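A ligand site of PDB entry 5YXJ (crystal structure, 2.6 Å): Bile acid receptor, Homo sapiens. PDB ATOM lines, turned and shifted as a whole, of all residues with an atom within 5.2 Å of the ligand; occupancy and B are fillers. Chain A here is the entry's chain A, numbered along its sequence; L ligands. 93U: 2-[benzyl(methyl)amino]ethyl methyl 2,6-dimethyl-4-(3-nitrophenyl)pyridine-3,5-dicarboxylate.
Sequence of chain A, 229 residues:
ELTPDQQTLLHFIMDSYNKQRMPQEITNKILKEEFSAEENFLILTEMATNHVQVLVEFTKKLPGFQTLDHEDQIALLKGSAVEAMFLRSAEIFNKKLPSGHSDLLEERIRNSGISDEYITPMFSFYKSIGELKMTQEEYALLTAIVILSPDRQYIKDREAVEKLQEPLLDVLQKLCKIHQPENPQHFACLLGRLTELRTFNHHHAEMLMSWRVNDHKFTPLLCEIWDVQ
ND1 of His 204 sits at hydrogen-bond distance from N of the ligand (2.8 Å).
N1 of the ligand lies close to NE2 of His 51, 3.2 Å away.
The side-chain hydroxyl of Tyr 126 sits at hydrogen-bond distance from the side-chain sulfur of Met 122, at 3.2 Å.
The backbone carbonyl oxygen (O) of Phe 86 lies within hydrogen-bond range of the side-chain hydroxyl (OG) of Ser 89.
The side-chain sulfur of Met 85 is in hydrogen-bond range of the indole nitrogen of Trp 226, 3.7 Å away.
The side-chain hydroxyl (OG) of Ser 89 is in hydrogen-bond range of the side-chain hydroxyl (OH) of Tyr 126, 2.7 Å away.
O2 of the ligand lies close to SD of Met 122, at 2.8 Å.
Residues that only touch the ligand: Met 207, Ile 119, Phe 86, Trp 226, Ser 89, Leu 208, Tyr 126, Ile 114, Met 85, Val 213, Ile 109, Leu 105, Val 82, Leu 44, Ala 48, Met 47 and Ile 92.
Hydrophobic or aromatic side chains within 4 Å of the ligand: Leu 44, Met 47, Ala 48, His 51, Val 82, Met 85, Phe 86, Leu 105, Ile 109, Ile 114, Ile 119, Met 122, His 204, Met 207, Leu 208, Val 213 and Trp 226.
Within 4 Å of the ligand: Leu 44, Met 47, Ala 48, His 51, Val 82, Met 85, Phe 86, Ser 89, Ile 92, Leu 105, Ile 109, Ile 114, Ile 119, Met 122, Tyr 126, His 204, Met 207, Leu 208, Val 213 and Trp 226.
The nearest printed residue that does not touch the ligand is Phe 41 (4.03 Å).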
ATOM      1  N   MET A  22     -20.189 -31.569  -1.427  1.00  0.00           N
ATOM      2  CA  MET A  22     -19.487 -30.284  -1.586  1.00  0.00           C
ATOM      3  C   MET A  22     -18.230 -30.232  -0.677  1.00  0.00           C
ATOM      4  O   MET A  22     -18.344 -30.408   0.543  1.00  0.00           O
ATOM      5  CB  MET A  22     -20.394 -29.078  -1.336  1.00  0.00           C
ATOM      6  CG  MET A  22     -19.635 -27.749  -1.459  1.00  0.00           C
ATOM      7  SD  MET A  22     -20.514 -26.381  -2.243  1.00  0.00           S
ATOM      8  CE  MET A  22     -21.705 -26.089  -0.944  1.00  0.00           C
ATOM      9  N   PHE A  41     -18.879 -13.199  -5.491  1.00  0.00           N
ATOM     10  CA  PHE A  41     -18.976 -13.768  -6.840  1.00  0.00           C
ATOM     11  C   PHE A  41     -17.958 -14.870  -7.089  1.00  0.00           C
ATOM     12  O   PHE A  41     -18.260 -15.848  -7.763  1.00  0.00           O
ATOM     13  CB  PHE A  41     -18.794 -12.715  -7.919  1.00  0.00           C
ATOM     14  CG  PHE A  41     -19.304 -13.136  -9.227  1.00  0.00           C
ATOM     15  CD1 PHE A  41     -20.656 -13.011  -9.504  1.00  0.00           C
ATOM     16  CD2 PHE A  41     -18.483 -13.714 -10.155  1.00  0.00           C
ATOM     17  CE1 PHE A  41     -21.198 -13.446 -10.720  1.00  0.00           C
ATOM     18  CE2 PHE A  41     -19.008 -14.174 -11.389  1.00  0.00           C
ATOM     19  CZ  PHE A  41     -20.371 -14.045 -11.673  1.00  0.00           C
ATOM     20  N   LEU A  44     -19.217 -18.136  -5.433  1.00  0.00           N
ATOM     21  CA  LEU A  44     -20.300 -18.746  -6.203  1.00  0.00           C
ATOM     22  C   LEU A  44     -19.738 -19.404  -7.426  1.00  0.00           C
ATOM     23  O   LEU A  44     -20.105 -20.532  -7.774  1.00  0.00           O
ATOM     24  CB  LEU A  44     -21.356 -17.741  -6.630  1.00  0.00           C
ATOM     25  CG  LEU A  44     -21.979 -16.858  -5.537  1.00  0.00           C
ATOM     26  CD1 LEU A  44     -22.808 -15.777  -6.202  1.00  0.00           C
ATOM     27  CD2 LEU A  44     -22.815 -17.662  -4.544  1.00  0.00           C
ATOM     28  N   THR A  45     -18.830 -18.709  -8.064  1.00  0.00           N
ATOM     29  CA  THR A  45     -18.077 -19.257  -9.183  1.00  0.00           C
ATOM     30  C   THR A  45     -17.435 -20.601  -8.825  1.00  0.00           C
ATOM     31  O   THR A  45     -17.737 -21.595  -9.449  1.00  0.00           O
ATOM     32  CB  THR A  45     -17.107 -18.166  -9.716  1.00  0.00           C
ATOM     33  OG1 THR A  45     -17.875 -17.248 -10.509  1.00  0.00           O
ATOM     34  CG2 THR A  45     -16.025 -18.753 -10.564  1.00  0.00           C
ATOM     35  N   MET A  47     -18.296 -22.623  -6.599  1.00  0.00           N
ATOM     36  CA  MET A  47     -19.322 -23.587  -6.227  1.00  0.00           C
ATOM     37  C   MET A  47     -19.975 -24.097  -7.497  1.00  0.00           C
ATOM     38  O   MET A  47     -20.180 -25.298  -7.651  1.00  0.00           O
ATOM     39  CB  MET A  47     -20.372 -23.005  -5.272  1.00  0.00           C
ATOM     40  CG  MET A  47     -19.912 -22.854  -3.837  1.00  0.00           C
ATOM     41  SD  MET A  47     -21.173 -21.918  -2.977  1.00  0.00           S
ATOM     42  CE  MET A  47     -20.386 -21.678  -1.421  1.00  0.00           C
ATOM     43  N   ALA A  48     -20.325 -23.181  -8.390  1.00  0.00           N
ATOM     44  CA  ALA A  48     -20.850 -23.573  -9.667  1.00  0.00           C
ATOM     45  C   ALA A  48     -19.884 -24.541 -10.320  1.00  0.00           C
ATOM     46  O   ALA A  48     -20.286 -25.617 -10.736  1.00  0.00           O
ATOM     47  CB  ALA A  48     -21.090 -22.348 -10.537  1.00  0.00           C
ATOM     48  N   HIS A  51     -20.285 -27.849  -8.820  1.00  0.00           N
ATOM     49  CA  HIS A  51     -21.552 -28.445  -9.275  1.00  0.00           C
ATOM     50  C   HIS A  51     -21.248 -29.281 -10.532  1.00  0.00           C
ATOM     51  O   HIS A  51     -21.668 -30.433 -10.637  1.00  0.00           O
ATOM     52  CB  HIS A  51     -22.661 -27.418  -9.608  1.00  0.00           C
ATOM     53  CG  HIS A  51     -23.168 -26.626  -8.451  1.00  0.00           C
ATOM     54  ND1 HIS A  51     -23.170 -27.090  -7.160  1.00  0.00           N
ATOM     55  CD2 HIS A  51     -23.748 -25.406  -8.401  1.00  0.00           C
ATOM     56  CE1 HIS A  51     -23.676 -26.175  -6.353  1.00  0.00           C
ATOM     57  NE2 HIS A  51     -24.037 -25.132  -7.079  1.00  0.00           N
ATOM     58  N   VAL A  82     -27.527 -26.873 -16.659  1.00  0.00           N
ATOM     59  CA  VAL A  82     -28.134 -25.757 -15.870  1.00  0.00           C
ATOM     60  C   VAL A  82     -29.179 -26.274 -14.869  1.00  0.00           C
ATOM     61  O   VAL A  82     -29.126 -25.941 -13.666  1.00  0.00           O
ATOM     62  CB  VAL A  82     -28.806 -24.712 -16.785  1.00  0.00           C
ATOM     63  CG1 VAL A  82     -29.517 -23.662 -15.965  1.00  0.00           C
ATOM     64  CG2 VAL A  82     -27.762 -24.021 -17.665  1.00  0.00           C
ATOM     65  N   MET A  85     -27.546 -28.402 -12.197  1.00  0.00           N
ATOM     66  CA  MET A  85     -26.770 -27.636 -11.206  1.00  0.00           C
ATOM     67  C   MET A  85     -27.650 -26.900 -10.246  1.00  0.00           C
ATOM     68  O   MET A  85     -27.337 -26.866  -9.056  1.00  0.00           O
ATOM     69  CB  MET A  85     -25.869 -26.610 -11.842  1.00  0.00           C
ATOM     70  CG  MET A  85     -24.707 -27.183 -12.641  1.00  0.00           C
ATOM     71  SD  MET A  85     -24.240 -25.932 -13.854  1.00  0.00           S
ATOM     72  CE  MET A  85     -23.265 -24.899 -12.754  1.00  0.00           C
ATOM     73  N   PHE A  86     -28.746 -26.287 -10.722  1.00  0.00           N
ATOM     74  CA  PHE A  86     -29.599 -25.598  -9.783  1.00  0.00           C
ATOM     75  C   PHE A  86     -30.153 -26.553  -8.828  1.00  0.00           C
ATOM     76  O   PHE A  86     -30.293 -26.196  -7.724  1.00  0.00           O
ATOM     77  CB  PHE A  86     -30.757 -24.802 -10.399  1.00  0.00           C
ATOM     78  CG  PHE A  86     -30.360 -23.410 -10.749  1.00  0.00           C
ATOM     79  CD1 PHE A  86     -30.236 -22.461  -9.786  1.00  0.00           C
ATOM     80  CD2 PHE A  86     -30.015 -23.098 -12.022  1.00  0.00           C
ATOM     81  CE1 PHE A  86     -29.806 -21.210 -10.093  1.00  0.00           C
ATOM     82  CE2 PHE A  86     -29.600 -21.833 -12.353  1.00  0.00           C
ATOM     83  CZ  PHE A  86     -29.483 -20.902 -11.376  1.00  0.00           C
ATOM     84  N   SER A  89     -27.646 -27.369  -6.056  1.00  0.00           N
ATOM     85  CA  SER A  89     -27.604 -26.223  -5.128  1.00  0.00           C
ATOM     86  C   SER A  89     -28.824 -26.158  -4.161  1.00  0.00           C
ATOM     87  O   SER A  89     -28.688 -25.764  -2.999  1.00  0.00           O
ATOM     88  CB  SER A  89     -27.434 -24.876  -5.864  1.00  0.00           C
ATOM     89  OG  SER A  89     -28.633 -24.441  -6.523  1.00  0.00           O
ATOM     90  N   ALA A  90     -30.011 -26.536  -4.650  1.00  0.00           N
ATOM     91  CA  ALA A  90     -31.207 -26.519  -3.831  1.00  0.00           C
ATOM     92  C   ALA A  90     -31.127 -27.571  -2.772  1.00  0.00           C
ATOM     93  O   ALA A  90     -31.500 -27.332  -1.626  1.00  0.00           O
ATOM     94  CB  ALA A  90     -32.446 -26.703  -4.667  1.00  0.00           C
ATOM     95  N   ILE A  92     -28.263 -28.646  -1.548  1.00  0.00           N
ATOM     96  CA  ILE A  92     -27.254 -28.123  -0.649  1.00  0.00           C
ATOM     97  C   ILE A  92     -27.657 -26.768  -0.036  1.00  0.00           C
ATOM     98  O   ILE A  92     -26.824 -26.118   0.552  1.00  0.00           O
ATOM     99  CB  ILE A  92     -25.930 -27.830  -1.344  1.00  0.00           C
ATOM    100  CG1 ILE A  92     -25.342 -29.044  -2.033  1.00  0.00           C
ATOM    101  CG2 ILE A  92     -24.880 -27.311  -0.339  1.00  0.00           C
ATOM    102  CD1 ILE A  92     -24.172 -28.660  -2.936  1.00  0.00           C
ATOM    103  N   PHE A  93     -28.871 -26.274  -0.193  1.00  0.00           N
ATOM    104  CA  PHE A  93     -29.305 -25.138   0.595  1.00  0.00           C
ATOM    105  C   PHE A  93     -30.337 -25.549   1.630  1.00  0.00           C
ATOM    106  O   PHE A  93     -30.273 -25.146   2.787  1.00  0.00           O
ATOM    107  CB  PHE A  93     -29.829 -24.063  -0.335  1.00  0.00           C
ATOM    108  CG  PHE A  93     -30.092 -22.794   0.352  1.00  0.00           C
ATOM    109  CD1 PHE A  93     -29.046 -21.951   0.701  1.00  0.00           C
ATOM    110  CD2 PHE A  93     -31.369 -22.468   0.744  1.00  0.00           C
ATOM    111  CE1 PHE A  93     -29.312 -20.786   1.412  1.00  0.00           C
ATOM    112  CE2 PHE A  93     -31.620 -21.302   1.429  1.00  0.00           C
ATOM    113  CZ  PHE A  93     -30.596 -20.464   1.768  1.00  0.00           C
ATOM    114  N   LEU A 105     -24.537 -17.675   3.342  1.00  0.00           N
ATOM    115  CA  LEU A 105     -24.462 -17.943   1.916  1.00  0.00           C
ATOM    116  C   LEU A 105     -25.495 -17.108   1.168  1.00  0.00           C
ATOM    117  O   LEU A 105     -25.179 -16.507   0.145  1.00  0.00           O
ATOM    118  CB  LEU A 105     -24.622 -19.454   1.590  1.00  0.00           C
ATOM    119  CG  LEU A 105     -24.470 -19.753   0.084  1.00  0.00           C
ATOM    120  CD1 LEU A 105     -23.181 -19.203  -0.553  1.00  0.00           C
ATOM    121  CD2 LEU A 105     -24.613 -21.229  -0.203  1.00  0.00           C
ATOM    122  N   ILE A 109     -24.783 -14.511  -1.649  1.00  0.00           N
ATOM    123  CA  ILE A 109     -25.539 -14.535  -2.915  1.00  0.00           C
ATOM    124  C   ILE A 109     -26.230 -13.183  -3.258  1.00  0.00           C
ATOM    125  O   ILE A 109     -26.242 -12.788  -4.421  1.00  0.00           O
ATOM    126  CB  ILE A 109     -26.612 -15.657  -2.914  1.00  0.00           C
ATOM    127  CG1 ILE A 109     -25.962 -17.018  -2.988  1.00  0.00           C
ATOM    128  CG2 ILE A 109     -27.589 -15.518  -4.090  1.00  0.00           C
ATOM    129  CD1 ILE A 109     -26.847 -18.135  -2.440  1.00  0.00           C
ATOM    130  N   ILE A 114     -25.148  -9.952  -8.594  1.00  0.00           N
ATOM    131  CA  ILE A 114     -26.148 -10.574  -9.458  1.00  0.00           C
ATOM    132  C   ILE A 114     -27.425  -9.868  -9.179  1.00  0.00           C
ATOM    133  O   ILE A 114     -27.764  -9.673  -8.019  1.00  0.00           O
ATOM    134  CB  ILE A 114     -26.321 -12.076  -9.171  1.00  0.00           C
ATOM    135  CG1 ILE A 114     -25.109 -12.862  -9.691  1.00  0.00           C
ATOM    136  CG2 ILE A 114     -27.566 -12.584  -9.873  1.00  0.00           C
ATOM    137  CD1 ILE A 114     -25.010 -14.310  -9.208  1.00  0.00           C
ATOM    138  N   TYR A 118     -32.743 -12.515 -11.166  1.00  0.00           N
ATOM    139  CA  TYR A 118     -32.237 -13.875 -11.093  1.00  0.00           C
ATOM    140  C   TYR A 118     -32.288 -14.470  -9.702  1.00  0.00           C
ATOM    141  O   TYR A 118     -32.916 -15.531  -9.503  1.00  0.00           O
ATOM    142  CB  TYR A 118     -30.805 -13.909 -11.644  1.00  0.00           C
ATOM    143  CG  TYR A 118     -30.738 -13.258 -12.995  1.00  0.00           C
ATOM    144  CD1 TYR A 118     -31.575 -13.691 -14.043  1.00  0.00           C
ATOM    145  CD2 TYR A 118     -29.911 -12.166 -13.218  1.00  0.00           C
ATOM    146  CE1 TYR A 118     -31.545 -13.069 -15.274  1.00  0.00           C
ATOM    147  CE2 TYR A 118     -29.862 -11.551 -14.457  1.00  0.00           C
ATOM    148  CZ  TYR A 118     -30.674 -11.998 -15.483  1.00  0.00           C
ATOM    149  OH  TYR A 118     -30.611 -11.393 -16.707  1.00  0.00           O
ATOM    150  N   ILE A 119     -31.687 -13.791  -8.734  1.00  0.00           N
ATOM    151  CA  ILE A 119     -31.745 -14.198  -7.307  1.00  0.00           C
ATOM    152  C   ILE A 119     -33.167 -14.498  -6.794  1.00  0.00           C
ATOM    153  O   ILE A 119     -33.348 -15.473  -6.069  1.00  0.00           O
ATOM    154  CB  ILE A 119     -31.167 -13.150  -6.302  1.00  0.00           C
ATOM    155  CG1 ILE A 119     -29.767 -12.641  -6.693  1.00  0.00           C
ATOM    156  CG2 ILE A 119     -31.191 -13.696  -4.878  1.00  0.00           C
ATOM    157  CD1 ILE A 119     -28.804 -13.729  -6.958  1.00  0.00           C
ATOM    158  N   MET A 122     -34.484 -17.942  -7.861  1.00  0.00           N
ATOM    159  CA  MET A 122     -33.594 -18.965  -7.293  1.00  0.00           C
ATOM    160  C   MET A 122     -34.122 -19.382  -5.925  1.00  0.00           C
ATOM    161  O   MET A 122     -34.325 -20.597  -5.656  1.00  0.00           O
ATOM    162  CB  MET A 122     -32.112 -18.479  -7.213  1.00  0.00           C
ATOM    163  CG  MET A 122     -31.101 -19.638  -7.084  1.00  0.00           C
ATOM    164  SD  MET A 122     -29.308 -19.356  -6.741  1.00  0.00           S
ATOM    165  CE  MET A 122     -29.382 -18.309  -5.320  1.00  0.00           C
ATOM    166  N   TYR A 126     -36.015 -22.657  -4.281  1.00  0.00           N
ATOM    167  CA  TYR A 126     -35.516 -23.430  -3.129  1.00  0.00           C
ATOM    168  C   TYR A 126     -36.636 -23.698  -2.113  1.00  0.00           C
ATOM    169  O   TYR A 126     -36.763 -24.837  -1.596  1.00  0.00           O
ATOM    170  CB  TYR A 126     -34.302 -22.795  -2.466  1.00  0.00           C
ATOM    171  CG  TYR A 126     -33.016 -22.663  -3.278  1.00  0.00           C
ATOM    172  CD1 TYR A 126     -32.796 -23.350  -4.481  1.00  0.00           C
ATOM    173  CD2 TYR A 126     -31.983 -21.880  -2.797  1.00  0.00           C
ATOM    174  CE1 TYR A 126     -31.600 -23.207  -5.175  1.00  0.00           C
ATOM    175  CE2 TYR A 126     -30.797 -21.715  -3.488  1.00  0.00           C
ATOM    176  CZ  TYR A 126     -30.614 -22.368  -4.664  1.00  0.00           C
ATOM    177  OH  TYR A 126     -29.412 -22.179  -5.275  1.00  0.00           O
ATOM    178  N   HIS A 204     -30.626 -18.435 -16.922  1.00  0.00           N
ATOM    179  CA  HIS A 204     -29.219 -18.685 -17.158  1.00  0.00           C
ATOM    180  C   HIS A 204     -28.648 -18.047 -18.434  1.00  0.00           C
ATOM    181  O   HIS A 204     -27.584 -17.383 -18.388  1.00  0.00           O
ATOM    182  CB  HIS A 204     -28.990 -20.178 -17.217  1.00  0.00           C
ATOM    183  CG  HIS A 204     -27.643 -20.567 -17.671  1.00  0.00           C
ATOM    184  ND1 HIS A 204     -26.538 -20.474 -16.858  1.00  0.00           N
ATOM    185  CD2 HIS A 204     -27.194 -21.023 -18.872  1.00  0.00           C
ATOM    186  CE1 HIS A 204     -25.465 -20.876 -17.518  1.00  0.00           C
ATOM    187  NE2 HIS A 204     -25.838 -21.218 -18.740  1.00  0.00           N
ATOM    188  N   MET A 207     -28.256 -14.279 -17.948  1.00  0.00           N
ATOM    189  CA  MET A 207     -27.118 -13.941 -17.085  1.00  0.00           C
ATOM    190  C   MET A 207     -25.849 -14.080 -17.860  1.00  0.00           C
ATOM    191  O   MET A 207     -25.117 -13.137 -17.961  1.00  0.00           O
ATOM    192  CB  MET A 207     -27.030 -14.881 -15.918  1.00  0.00           C
ATOM    193  CG  MET A 207     -28.098 -14.616 -14.882  1.00  0.00           C
ATOM    194  SD  MET A 207     -27.855 -15.816 -13.578  1.00  0.00           S
ATOM    195  CE  MET A 207     -26.249 -15.318 -12.911  1.00  0.00           C
ATOM    196  N   LEU A 208     -25.619 -15.203 -18.494  1.00  0.00           N
ATOM    197  CA  LEU A 208     -24.424 -15.336 -19.331  1.00  0.00           C
ATOM    198  C   LEU A 208     -24.147 -14.096 -20.161  1.00  0.00           C
ATOM    199  O   LEU A 208     -23.025 -13.620 -20.197  1.00  0.00           O
ATOM    200  CB  LEU A 208     -24.471 -16.560 -20.243  1.00  0.00           C
ATOM    201  CG  LEU A 208     -23.671 -17.724 -19.735  1.00  0.00           C
ATOM    202  CD1 LEU A 208     -24.083 -18.127 -18.348  1.00  0.00           C
ATOM    203  CD2 LEU A 208     -23.903 -18.906 -20.655  1.00  0.00           C
ATOM    204  N   VAL A 213     -22.124 -10.447 -15.347  1.00  0.00           N
ATOM    205  CA  VAL A 213     -21.894 -11.900 -15.501  1.00  0.00           C
ATOM    206  C   VAL A 213     -20.993 -12.267 -16.724  1.00  0.00           C
ATOM    207  O   VAL A 213     -20.242 -13.248 -16.651  1.00  0.00           O
ATOM    208  CB  VAL A 213     -23.226 -12.705 -15.582  1.00  0.00           C
ATOM    209  CG1 VAL A 213     -22.963 -14.206 -15.572  1.00  0.00           C
ATOM    210  CG2 VAL A 213     -24.196 -12.340 -14.451  1.00  0.00           C
ATOM    211  N   PHE A 218     -14.922 -17.286 -16.582  1.00  0.00           N
ATOM    212  CA  PHE A 218     -15.411 -18.441 -15.835  1.00  0.00           C
ATOM    213  C   PHE A 218     -14.344 -19.526 -15.828  1.00  0.00           C
ATOM    214  O   PHE A 218     -13.494 -19.524 -16.693  1.00  0.00           O
ATOM    215  CB  PHE A 218     -16.738 -18.933 -16.429  1.00  0.00           C
ATOM    216  CG  PHE A 218     -17.883 -17.971 -16.220  1.00  0.00           C
ATOM    217  CD1 PHE A 218     -18.189 -17.504 -14.914  1.00  0.00           C
ATOM    218  CD2 PHE A 218     -18.664 -17.546 -17.299  1.00  0.00           C
ATOM    219  CE1 PHE A 218     -19.232 -16.634 -14.720  1.00  0.00           C
ATOM    220  CE2 PHE A 218     -19.696 -16.658 -17.097  1.00  0.00           C
ATOM    221  CZ  PHE A 218     -19.984 -16.200 -15.800  1.00  0.00           C
ATOM    222  N   TRP A 226     -21.081 -24.682 -20.645  1.00  0.00           N
ATOM    223  CA  TRP A 226     -22.120 -23.636 -20.877  1.00  0.00           C
ATOM    224  C   TRP A 226     -21.987 -22.987 -22.254  1.00  0.00           C
ATOM    225  O   TRP A 226     -22.597 -21.966 -22.486  1.00  0.00           O
ATOM    226  CB  TRP A 226     -22.061 -22.500 -19.807  1.00  0.00           C
ATOM    227  CG  TRP A 226     -22.564 -22.748 -18.396  1.00  0.00           C
ATOM    228  CD1 TRP A 226     -23.468 -23.703 -17.975  1.00  0.00           C
ATOM    229  CD2 TRP A 226     -22.203 -22.005 -17.237  1.00  0.00           C
ATOM    230  NE1 TRP A 226     -23.667 -23.608 -16.632  1.00  0.00           N
ATOM    231  CE2 TRP A 226     -22.933 -22.566 -16.140  1.00  0.00           C
ATOM    232  CE3 TRP A 226     -21.357 -20.915 -16.999  1.00  0.00           C
ATOM    233  CZ2 TRP A 226     -22.841 -22.058 -14.824  1.00  0.00           C
ATOM    234  CZ3 TRP A 226     -21.232 -20.407 -15.666  1.00  0.00           C
ATOM    235  CH2 TRP A 226     -21.978 -20.984 -14.599  1.00  0.00           C
HETATM  236  C1  93U L   1     -24.809 -19.261 -13.960  1.00  0.00           C
HETATM  237  O1  93U L   1     -26.715 -21.610  -9.553  1.00  0.00           O
HETATM  238  O2  93U L   1     -28.644 -16.702  -7.498  1.00  0.00           O
HETATM  239  C2  93U L   1     -24.531 -18.894 -12.540  1.00  0.00           C
HETATM  240  C3  93U L   1     -25.103 -19.716 -11.448  1.00  0.00           C
HETATM  241  C4  93U L   1     -25.758 -21.001 -11.883  1.00  0.00           C
HETATM  242  C5  93U L   1     -25.952 -21.281 -13.329  1.00  0.00           C
HETATM  243  O3  93U L   1     -26.319 -16.976  -7.263  1.00  0.00           O
HETATM  244  O4  93U L   1     -23.388 -16.798 -12.953  1.00  0.00           O
HETATM  245  O5  93U L   1     -23.476 -17.530 -10.780  1.00  0.00           O
HETATM  246  C24 93U L   1     -23.796 -17.658 -12.173  1.00  0.00           C
HETATM  247  C25 93U L   1     -22.123 -17.424 -10.362  1.00  0.00           C
HETATM  248  C18 93U L   1     -26.286 -18.884 -11.037  1.00  0.00           C
HETATM  249  C23 93U L   1     -27.384 -18.609 -11.877  1.00  0.00           C
HETATM  250  C22 93U L   1     -28.502 -17.842 -11.503  1.00  0.00           C
HETATM  251  C21 93U L   1     -28.539 -17.338 -10.222  1.00  0.00           C
HETATM  252  C20 93U L   1     -27.451 -17.600  -9.383  1.00  0.00           C
HETATM  253  N2  93U L   1     -27.442 -17.093  -8.073  1.00  0.00           N
HETATM  254  C19 93U L   1     -26.359 -18.353  -9.778  1.00  0.00           C
HETATM  255  C6  93U L   1     -26.666 -22.514 -13.850  1.00  0.00           C
HETATM  256  N   93U L   1     -25.478 -20.401 -14.240  1.00  0.00           N
HETATM  257  C   93U L   1     -24.343 -18.438 -15.122  1.00  0.00           C
HETATM  258  C7  93U L   1     -26.261 -21.966 -10.875  1.00  0.00           C
HETATM  259  O   93U L   1     -26.200 -23.127 -11.121  1.00  0.00           O
HETATM  260  C8  93U L   1     -26.576 -22.514  -8.482  1.00  0.00           C
HETATM  261  C9  93U L   1     -26.103 -21.671  -7.313  1.00  0.00           C
HETATM  262  N1  93U L   1     -24.710 -22.014  -6.957  1.00  0.00           N
HETATM  263  C10 93U L   1     -23.829 -21.444  -8.010  1.00  0.00           C
HETATM  264  C11 93U L   1     -24.357 -21.490  -5.605  1.00  0.00           C
HETATM  265  C12 93U L   1     -25.047 -22.240  -4.483  1.00  0.00           C
HETATM  266  C17 93U L   1     -26.175 -21.686  -3.925  1.00  0.00           C
HETATM  267  C16 93U L   1     -26.863 -22.349  -2.941  1.00  0.00           C
HETATM  268  C15 93U L   1     -26.418 -23.593  -2.486  1.00  0.00           C
HETATM  269  C14 93U L   1     -25.281 -24.168  -3.047  1.00  0.00           C
HETATM  270  C13 93U L   1     -24.597 -23.483  -4.052  1.00  0.00           C
